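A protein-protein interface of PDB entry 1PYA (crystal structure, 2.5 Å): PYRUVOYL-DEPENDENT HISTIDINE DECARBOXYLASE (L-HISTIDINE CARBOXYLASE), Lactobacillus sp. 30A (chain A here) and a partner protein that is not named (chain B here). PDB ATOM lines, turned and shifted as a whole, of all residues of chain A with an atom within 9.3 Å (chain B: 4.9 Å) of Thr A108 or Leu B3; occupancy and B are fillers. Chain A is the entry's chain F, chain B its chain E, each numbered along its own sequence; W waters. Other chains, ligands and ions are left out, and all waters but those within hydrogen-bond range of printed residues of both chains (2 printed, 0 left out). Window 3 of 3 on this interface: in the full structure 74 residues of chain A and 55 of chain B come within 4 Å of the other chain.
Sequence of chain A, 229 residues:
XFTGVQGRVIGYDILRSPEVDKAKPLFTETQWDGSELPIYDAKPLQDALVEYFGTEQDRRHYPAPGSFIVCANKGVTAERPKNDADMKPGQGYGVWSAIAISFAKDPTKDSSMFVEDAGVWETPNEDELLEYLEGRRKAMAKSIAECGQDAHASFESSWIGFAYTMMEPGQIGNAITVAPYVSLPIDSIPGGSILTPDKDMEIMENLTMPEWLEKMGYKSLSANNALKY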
ATOM      1  N   THR A   3      -2.603  22.842 -18.600  1.00  0.00           N
ATOM      2  CA  THR A   3      -1.413  22.133 -18.155  1.00  0.00           C
ATOM      3  C   THR A   3      -1.581  20.746 -18.794  1.00  0.00           C
ATOM      4  O   THR A   3      -2.593  20.056 -18.602  1.00  0.00           O
ATOM      5  CB  THR A   3      -1.349  22.136 -16.592  1.00  0.00           C
ATOM      6  OG1 THR A   3      -0.146  21.396 -16.328  1.00  0.00           O
ATOM      7  CG2 THR A   3      -2.552  21.645 -15.873  1.00  0.00           C
ATOM      8  N   GLY A   4      -0.650  20.387 -19.673  1.00  0.00           N
ATOM      9  CA  GLY A   4      -0.882  19.223 -20.498  1.00  0.00           C
ATOM     10  C   GLY A   4       0.126  18.130 -20.342  1.00  0.00           C
ATOM     11  O   GLY A   4       0.590  17.824 -19.241  1.00  0.00           O
ATOM     12  N   VAL A   5       0.570  17.632 -21.489  1.00  0.00           N
ATOM     13  CA  VAL A   5       1.473  16.489 -21.506  1.00  0.00           C
ATOM     14  C   VAL A   5       2.791  16.739 -20.815  1.00  0.00           C
ATOM     15  O   VAL A   5       3.465  15.778 -20.449  1.00  0.00           O
ATOM     16  CB  VAL A   5       1.775  15.994 -22.952  1.00  0.00           C
ATOM     17  CG1 VAL A   5       0.489  15.318 -23.479  1.00  0.00           C
ATOM     18  CG2 VAL A   5       2.253  17.124 -23.869  1.00  0.00           C
ATOM     19  N   GLN A   6       3.206  18.002 -20.639  1.00  0.00           N
ATOM     20  CA  GLN A   6       4.476  18.345 -19.976  1.00  0.00           C
ATOM     21  C   GLN A   6       4.296  18.679 -18.502  1.00  0.00           C
ATOM     22  O   GLN A   6       5.318  18.906 -17.846  1.00  0.00           O
ATOM     23  CB  GLN A   6       5.139  19.569 -20.584  1.00  0.00           C
ATOM     24  CG  GLN A   6       5.566  19.448 -22.010  1.00  0.00           C
ATOM     25  CD  GLN A   6       5.677  20.819 -22.684  1.00  0.00           C
ATOM     26  OE1 GLN A   6       4.735  21.273 -23.372  1.00  0.00           O
ATOM     27  NE2 GLN A   6       6.802  21.508 -22.620  1.00  0.00           N
ATOM     28  N   GLY A   7       3.091  18.710 -17.918  1.00  0.00           N
ATOM     29  CA  GLY A   7       2.993  19.255 -16.586  1.00  0.00           C
ATOM     30  C   GLY A   7       2.543  18.306 -15.498  1.00  0.00           C
ATOM     31  O   GLY A   7       1.956  17.247 -15.726  1.00  0.00           O
ATOM     32  N   ARG A   8       2.886  18.786 -14.307  1.00  0.00           N
ATOM     33  CA  ARG A   8       2.463  18.200 -13.052  1.00  0.00           C
ATOM     34  C   ARG A   8       1.970  19.394 -12.219  1.00  0.00           C
ATOM     35  O   ARG A   8       2.387  20.539 -12.440  1.00  0.00           O
ATOM     36  CB  ARG A   8       3.654  17.432 -12.344  1.00  0.00           C
ATOM     37  CG  ARG A   8       3.717  16.007 -12.908  1.00  0.00           C
ATOM     38  CD  ARG A   8       4.595  14.914 -12.252  1.00  0.00           C
ATOM     39  NE  ARG A   8       5.907  15.183 -12.732  1.00  0.00           N
ATOM     40  CZ  ARG A   8       6.731  14.355 -13.358  1.00  0.00           C
ATOM     41  NH1 ARG A   8       6.608  13.049 -13.462  1.00  0.00           N
ATOM     42  NH2 ARG A   8       7.809  14.941 -13.844  1.00  0.00           N
ATOM     43  N   ASP A  13      -0.158  16.030  -8.232  1.00  0.00           N
ATOM     44  CA  ASP A  13       0.732  15.140  -8.936  1.00  0.00           C
ATOM     45  C   ASP A  13       2.064  15.015  -8.262  1.00  0.00           C
ATOM     46  O   ASP A  13       2.710  13.993  -8.429  1.00  0.00           O
ATOM     47  CB  ASP A  13       1.061  15.601 -10.320  1.00  0.00           C
ATOM     48  CG  ASP A  13      -0.069  15.683 -11.306  1.00  0.00           C
ATOM     49  OD1 ASP A  13      -0.707  14.678 -11.594  1.00  0.00           O
ATOM     50  OD2 ASP A  13      -0.312  16.770 -11.795  1.00  0.00           O
ATOM     51  N   PHE A 103      -8.768  18.038 -14.248  1.00  0.00           N
ATOM     52  CA  PHE A 103      -7.810  17.026 -14.683  1.00  0.00           C
ATOM     53  C   PHE A 103      -8.333  16.132 -15.800  1.00  0.00           C
ATOM     54  O   PHE A 103      -9.440  15.603 -15.708  1.00  0.00           O
ATOM     55  CB  PHE A 103      -7.419  16.205 -13.492  1.00  0.00           C
ATOM     56  CG  PHE A 103      -6.569  17.027 -12.537  1.00  0.00           C
ATOM     57  CD1 PHE A 103      -5.276  17.355 -12.882  1.00  0.00           C
ATOM     58  CD2 PHE A 103      -7.110  17.496 -11.361  1.00  0.00           C
ATOM     59  CE1 PHE A 103      -4.513  18.146 -12.054  1.00  0.00           C
ATOM     60  CE2 PHE A 103      -6.343  18.287 -10.530  1.00  0.00           C
ATOM     61  CZ  PHE A 103      -5.042  18.607 -10.875  1.00  0.00           C
ATOM     62  N   ALA A 104      -7.570  15.953 -16.874  1.00  0.00           N
ATOM     63  CA  ALA A 104      -8.023  15.179 -18.021  1.00  0.00           C
ATOM     64  C   ALA A 104      -8.053  13.678 -17.663  1.00  0.00           C
ATOM     65  O   ALA A 104      -7.154  13.203 -16.944  1.00  0.00           O
ATOM     66  CB  ALA A 104      -7.060  15.425 -19.186  1.00  0.00           C
ATOM     67  N   LYS A 105      -9.098  12.939 -18.086  1.00  0.00           N
ATOM     68  CA  LYS A 105      -9.149  11.482 -17.880  1.00  0.00           C
ATOM     69  C   LYS A 105      -8.009  10.817 -18.668  1.00  0.00           C
ATOM     70  O   LYS A 105      -7.349   9.907 -18.184  1.00  0.00           O
ATOM     71  CB  LYS A 105     -10.442  10.848 -18.375  1.00  0.00           C
ATOM     72  CG  LYS A 105     -11.579  10.881 -17.389  1.00  0.00           C
ATOM     73  CD  LYS A 105     -12.884  10.423 -18.050  1.00  0.00           C
ATOM     74  CE  LYS A 105     -13.998  10.535 -17.036  1.00  0.00           C
ATOM     75  NZ  LYS A 105     -15.290  10.596 -17.672  1.00  0.00           N
ATOM     76  N   ASP A 106      -7.704  11.240 -19.878  1.00  0.00           N
ATOM     77  CA  ASP A 106      -6.568  10.699 -20.592  1.00  0.00           C
ATOM     78  C   ASP A 106      -5.491  11.760 -20.845  1.00  0.00           C
ATOM     79  O   ASP A 106      -5.457  12.342 -21.923  1.00  0.00           O
ATOM     80  CB  ASP A 106      -7.060  10.096 -21.904  1.00  0.00           C
ATOM     81  CG  ASP A 106      -5.982   9.402 -22.748  1.00  0.00           C
ATOM     82  OD1 ASP A 106      -4.854   9.147 -22.289  1.00  0.00           O
ATOM     83  OD2 ASP A 106      -6.281   9.124 -23.907  1.00  0.00           O
ATOM     84  N   PRO A 107      -4.521  12.001 -19.964  1.00  0.00           N
ATOM     85  CA  PRO A 107      -3.475  13.000 -20.123  1.00  0.00           C
ATOM     86  C   PRO A 107      -2.506  12.749 -21.273  1.00  0.00           C
ATOM     87  O   PRO A 107      -1.597  13.560 -21.478  1.00  0.00           O
ATOM     88  CB  PRO A 107      -2.735  13.027 -18.810  1.00  0.00           C
ATOM     89  CG  PRO A 107      -3.612  12.245 -17.872  1.00  0.00           C
ATOM     90  CD  PRO A 107      -4.248  11.218 -18.774  1.00  0.00           C
ATOM     91  N   THR A 108      -2.596  11.654 -22.025  1.00  0.00           N
ATOM     92  CA  THR A 108      -1.683  11.498 -23.152  1.00  0.00           C
ATOM     93  C   THR A 108      -2.361  12.130 -24.340  1.00  0.00           C
ATOM     94  O   THR A 108      -1.704  12.364 -25.343  1.00  0.00           O
ATOM     95  CB  THR A 108      -1.370   9.983 -23.454  1.00  0.00           C
ATOM     96  OG1 THR A 108      -2.607   9.279 -23.653  1.00  0.00           O
ATOM     97  CG2 THR A 108      -0.604   9.322 -22.296  1.00  0.00           C
ATOM     98  N   LYS A 109      -3.675  12.358 -24.322  1.00  0.00           N
ATOM     99  CA  LYS A 109      -4.332  12.940 -25.480  1.00  0.00           C
ATOM    100  C   LYS A 109      -4.881  14.312 -25.184  1.00  0.00           C
ATOM    101  O   LYS A 109      -4.821  15.205 -26.017  1.00  0.00           O
ATOM    102  CB  LYS A 109      -5.493  12.068 -25.978  1.00  0.00           C
ATOM    103  CG  LYS A 109      -4.947  10.730 -26.450  1.00  0.00           C
ATOM    104  CD  LYS A 109      -5.925   9.894 -27.259  1.00  0.00           C
ATOM    105  CE  LYS A 109      -5.330   8.503 -27.462  1.00  0.00           C
ATOM    106  NZ  LYS A 109      -5.229   7.777 -26.199  1.00  0.00           N
ATOM    107  N   ASP A 110      -5.427  14.495 -24.004  1.00  0.00           N
ATOM    108  CA  ASP A 110      -6.089  15.730 -23.674  1.00  0.00           C
ATOM    109  C   ASP A 110      -5.292  16.478 -22.640  1.00  0.00           C
ATOM    110  O   ASP A 110      -4.714  15.894 -21.715  1.00  0.00           O
ATOM    111  CB  ASP A 110      -7.486  15.480 -23.099  1.00  0.00           C
ATOM    112  CG  ASP A 110      -8.445  14.784 -24.055  1.00  0.00           C
ATOM    113  OD1 ASP A 110      -8.461  15.097 -25.242  1.00  0.00           O
ATOM    114  OD2 ASP A 110      -9.201  13.934 -23.613  1.00  0.00           O
ATOM    115  N   SER A 111      -5.265  17.782 -22.820  1.00  0.00           N
ATOM    116  CA  SER A 111      -4.700  18.622 -21.788  1.00  0.00           C
ATOM    117  C   SER A 111      -5.721  18.810 -20.655  1.00  0.00           C
ATOM    118  O   SER A 111      -6.952  18.751 -20.829  1.00  0.00           O
ATOM    119  CB  SER A 111      -4.343  19.972 -22.398  1.00  0.00           C
ATOM    120  OG  SER A 111      -3.639  20.781 -21.475  1.00  0.00           O
ATOM    121  N   SER A 112      -5.154  18.973 -19.466  1.00  0.00           N
ATOM    122  CA  SER A 112      -5.879  19.422 -18.299  1.00  0.00           C
ATOM    123  C   SER A 112      -6.071  20.929 -18.433  1.00  0.00           C
ATOM    124  O   SER A 112      -5.235  21.639 -19.000  1.00  0.00           O
ATOM    125  CB  SER A 112      -5.065  19.098 -17.087  1.00  0.00           C
ATOM    126  OG  SER A 112      -5.248  17.722 -16.842  1.00  0.00           O
ATOM    127  N   GLU A 202      10.637  11.840 -10.022  1.00  0.00           N
ATOM    128  CA  GLU A 202      10.029  10.677  -9.391  1.00  0.00           C
ATOM    129  C   GLU A 202       9.977  10.752  -7.892  1.00  0.00           C
ATOM    130  O   GLU A 202       8.944  10.418  -7.274  1.00  0.00           O
ATOM    131  CB  GLU A 202      10.748   9.426  -9.738  1.00  0.00           C
ATOM    132  CG  GLU A 202      10.251   9.022 -11.111  1.00  0.00           C
ATOM    133  CD  GLU A 202      10.528   7.567 -11.478  1.00  0.00           C
ATOM    134  OE1 GLU A 202      10.719   6.730 -10.585  1.00  0.00           O
ATOM    135  OE2 GLU A 202      10.547   7.269 -12.675  1.00  0.00           O
ATOM    136  N   GLU A 205       7.030  13.004  -7.063  1.00  0.00           N
ATOM    137  CA  GLU A 205       5.780  12.299  -7.310  1.00  0.00           C
ATOM    138  C   GLU A 205       5.470  11.390  -6.145  1.00  0.00           C
ATOM    139  O   GLU A 205       4.324  11.250  -5.751  1.00  0.00           O
ATOM    140  CB  GLU A 205       5.832  11.376  -8.493  1.00  0.00           C
ATOM    141  CG  GLU A 205       5.871  12.064  -9.795  1.00  0.00           C
ATOM    142  CD  GLU A 205       5.717  11.118 -10.964  1.00  0.00           C
ATOM    143  OE1 GLU A 205       6.414  10.121 -11.062  1.00  0.00           O
ATOM    144  OE2 GLU A 205       4.903  11.419 -11.823  1.00  0.00           O
ATOM    145  N   SER B   1       5.925   8.218 -13.172  1.00  0.00           N
ATOM    146  CA  SER B   1       4.685   7.483 -13.287  1.00  0.00           C
ATOM    147  C   SER B   1       4.700   6.634 -14.516  1.00  0.00           C
ATOM    148  O   SER B   1       5.516   6.889 -15.389  1.00  0.00           O
ATOM    149  CB  SER B   1       3.513   8.421 -13.408  1.00  0.00           C
ATOM    150  OG  SER B   1       3.631   9.057 -12.168  1.00  0.00           O
ATOM    151  N   GLU B   2       3.721   5.732 -14.573  1.00  0.00           N
ATOM    152  CA  GLU B   2       3.477   4.899 -15.739  1.00  0.00           C
ATOM    153  C   GLU B   2       3.115   5.812 -16.905  1.00  0.00           C
ATOM    154  O   GLU B   2       3.405   5.477 -18.054  1.00  0.00           O
ATOM    155  CB  GLU B   2       2.328   3.949 -15.422  1.00  0.00           C
ATOM    156  CG  GLU B   2       2.400   2.582 -16.102  1.00  0.00           C
ATOM    157  CD  GLU B   2       1.567   2.436 -17.376  1.00  0.00           C
ATOM    158  OE1 GLU B   2       2.053   2.821 -18.448  1.00  0.00           O
ATOM    159  OE2 GLU B   2       0.442   1.917 -17.289  1.00  0.00           O
ATOM    160  N   LEU B   3       2.542   6.999 -16.585  1.00  0.00           N
ATOM    161  CA  LEU B   3       2.194   8.006 -17.581  1.00  0.00           C
ATOM    162  C   LEU B   3       3.435   8.454 -18.318  1.00  0.00           C
ATOM    163  O   LEU B   3       3.438   8.516 -19.555  1.00  0.00           O
ATOM    164  CB  LEU B   3       1.538   9.228 -16.935  1.00  0.00           C
ATOM    165  CG  LEU B   3       1.044  10.368 -17.837  1.00  0.00           C
ATOM    166  CD1 LEU B   3       0.051   9.849 -18.845  1.00  0.00           C
ATOM    167  CD2 LEU B   3       0.381  11.432 -16.987  1.00  0.00           C
ATOM    168  N   ASP B   4       4.504   8.675 -17.557  1.00  0.00           N
ATOM    169  CA  ASP B   4       5.747   9.099 -18.144  1.00  0.00           C
ATOM    170  C   ASP B   4       6.305   8.074 -19.116  1.00  0.00           C
ATOM    171  O   ASP B   4       6.872   8.481 -20.138  1.00  0.00           O
ATOM    172  CB  ASP B   4       6.716   9.405 -17.012  1.00  0.00           C
ATOM    173  CG  ASP B   4       6.305  10.653 -16.228  1.00  0.00           C
ATOM    174  OD1 ASP B   4       6.358  11.742 -16.787  1.00  0.00           O
ATOM    175  OD2 ASP B   4       5.928  10.539 -15.070  1.00  0.00           O
ATOM    176  N   ALA B   5       6.063   6.771 -18.927  1.00  0.00           N
ATOM    177  CA  ALA B   5       6.522   5.784 -19.882  1.00  0.00           C
ATOM    178  C   ALA B   5       5.794   5.949 -21.190  1.00  0.00           C
ATOM    179  O   ALA B   5       6.413   5.851 -22.255  1.00  0.00           O
ATOM    180  CB  ALA B   5       6.245   4.376 -19.425  1.00  0.00           C
ATOM    181  N   LYS B   6       4.490   6.219 -21.153  1.00  0.00           N
ATOM    182  CA  LYS B   6       3.678   6.398 -22.370  1.00  0.00           C
ATOM    183  C   LYS B   6       4.042   7.687 -23.101  1.00  0.00           C
ATOM    184  O   LYS B   6       4.170   7.715 -24.321  1.00  0.00           O
ATOM    185  CB  LYS B   6       2.215   6.440 -22.009  1.00  0.00           C
ATOM    186  CG  LYS B   6       1.761   5.264 -21.155  1.00  0.00           C
ATOM    187  CD  LYS B   6       0.239   5.295 -21.113  1.00  0.00           C
ATOM    188  CE  LYS B   6      -0.373   4.525 -19.942  1.00  0.00           C
ATOM    189  NZ  LYS B   6      -0.210   3.089 -20.097  1.00  0.00           N
ATOM    190  N   LEU B   7       4.305   8.736 -22.328  1.00  0.00           N
ATOM    191  CA  LEU B   7       4.690  10.079 -22.747  1.00  0.00           C
ATOM    192  C   LEU B   7       6.056  10.127 -23.410  1.00  0.00           C
ATOM    193  O   LEU B   7       6.238  10.663 -24.521  1.00  0.00           O
ATOM    194  CB  LEU B   7       4.615  10.944 -21.487  1.00  0.00           C
ATOM    195  CG  LEU B   7       3.570  12.072 -21.411  1.00  0.00           C
ATOM    196  CD1 LEU B   7       2.276  11.765 -22.154  1.00  0.00           C
ATOM    197  CD2 LEU B   7       3.333  12.330 -19.943  1.00  0.00           C
ATOM    198  N   LEU B  10       6.421   9.306 -27.007  1.00  0.00           N
ATOM    199  CA  LEU B  10       5.957  10.325 -27.928  1.00  0.00           C
ATOM    200  C   LEU B  10       7.000  11.430 -28.060  1.00  0.00           C
ATOM    201  O   LEU B  10       6.858  12.342 -28.873  1.00  0.00           O
ATOM    202  CB  LEU B  10       4.655  10.897 -27.415  1.00  0.00           C
ATOM    203  CG  LEU B  10       3.479   9.961 -27.155  1.00  0.00           C
ATOM    204  CD1 LEU B  10       2.338  10.800 -26.612  1.00  0.00           C
ATOM    205  CD2 LEU B  10       3.091   9.192 -28.425  1.00  0.00           C
ATOM    206  N   ARG B  14       8.369  15.231 -18.704  1.00  0.00           N
ATOM    207  CA  ARG B  14       7.863  16.214 -17.782  1.00  0.00           C
ATOM    208  C   ARG B  14       8.923  16.639 -16.787  1.00  0.00           C
ATOM    209  O   ARG B  14       8.605  17.028 -15.672  1.00  0.00           O
ATOM    210  CB  ARG B  14       6.631  15.635 -17.060  1.00  0.00           C
ATOM    211  CG  ARG B  14       5.569  15.035 -17.998  1.00  0.00           C
ATOM    212  CD  ARG B  14       4.276  14.892 -17.236  1.00  0.00           C
ATOM    213  NE  ARG B  14       4.376  13.813 -16.288  1.00  0.00           N
ATOM    214  CZ  ARG B  14       3.353  13.426 -15.527  1.00  0.00           C
ATOM    215  NH1 ARG B  14       2.212  14.112 -15.474  1.00  0.00           N
ATOM    216  NH2 ARG B  14       3.508  12.360 -14.750  1.00  0.00           N
HETATM  217  O   HOH W   1       6.611  18.124 -14.481  1.00  0.00           O
HETATM  218  O   HOH W   2       0.278  14.970 -18.188  1.00  0.00           O
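Thr A108 touches just these residues of chain B: Leu B3 and Leu B7. Leu B3 touches two residues of chain A. Of chain A, only Arg A8 and Glu A205 come within 4 Å of Asp B4. Of the printed residues of chain A, Leu B7 touches Val A5 and Thr A108. Of the printed residues of chain B, Val A5 touches Leu B7 and Arg B14. Printed residues of chain B within 4 Å of Gly A7: Arg B14. Printed residues of chain B within 4 Å of Pro A107: Leu B3.
Water W1 lies within hydrogen-bond range of O of Arg B14 (2.6 Å) and NH2 of Arg A8 (3.5 Å). Water W2 bridges the backbone carbonyl oxygen of Gly A4 (3.1 Å) and the guanidinium group of Arg B14 (3.4 Å).
The backbone NH of Ser B1 sits at hydrogen-bond distance from the side-chain carboxylate of Asp B4 (3.0 Å). The guanidinium group (NE) of Arg B14 is in salt-bridge range of the side-chain carboxylate (OD1) of Asp B4, 2.9 Å away. NH1 of Arg A8 lies within salt-bridge range of OE2 of Glu A205, at 2.9 Å. OD1 of Asp A106 lies within hydrogen-bond range of OG1 of Thr A108 (2.6 Å).
Among the printed residues, pairs that only touch across the chains: Val A5 with Arg B14 (3.3 Å), Val A5 with Leu B7 (3.5 Å), Glu A205 with Asp B4 (3.5 Å), Thr A108 with Leu B3 (3.6 Å), Gln A6 with Arg B14 (3.6 Å), Thr A108 with Leu B7 (3.8 Å) and Pro A107 with Leu B3 (3.9 Å).
Of the 9 printed residues of chain B, 5 touch a printed residue of chain A. Hydrophobic or aromatic side chains of chain B within 4 Å of the printed part of chain A: Leu B3 and Leu B7. Of the 19 printed residues of chain A, 7 touch a printed residue of chain B. Printed residues of chain A that touch a printed residue of chain B: Val A5, Gln A6, Gly A7, Arg A8, Pro A107, Thr A108 and Glu A205. Hydrophobic or aromatic side chains of chain A within 4 Å of the printed part of chain B: Pro A107. Among the printed residues, Asp or Glu carboxylates within 4 Å of a Lys or Arg side-chain nitrogen of the other chain: Arg A8 with Asp B4 (3.1 Å) and Glu A205 with Arg B14 (3.4 Å).
OE2 of Glu A205 lies within hydrogen-bond range of OG of Ser B1 (2.7 Å). The guanidinium group (NH1) of Arg A8 lies within salt-bridge range of the side-chain carboxylate (OD2) of Asp B4, at 3.1 Å. The backbone carbonyl oxygen of Gly A7 sits at hydrogen-bond distance from the guanidinium group of Arg B14. NH2 of Arg A8 is in hydrogen-bond range of O of Arg B14. NH2 of Arg B14 lies within salt-bridge range of OE2 of Glu A205, at 3.4 Å.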
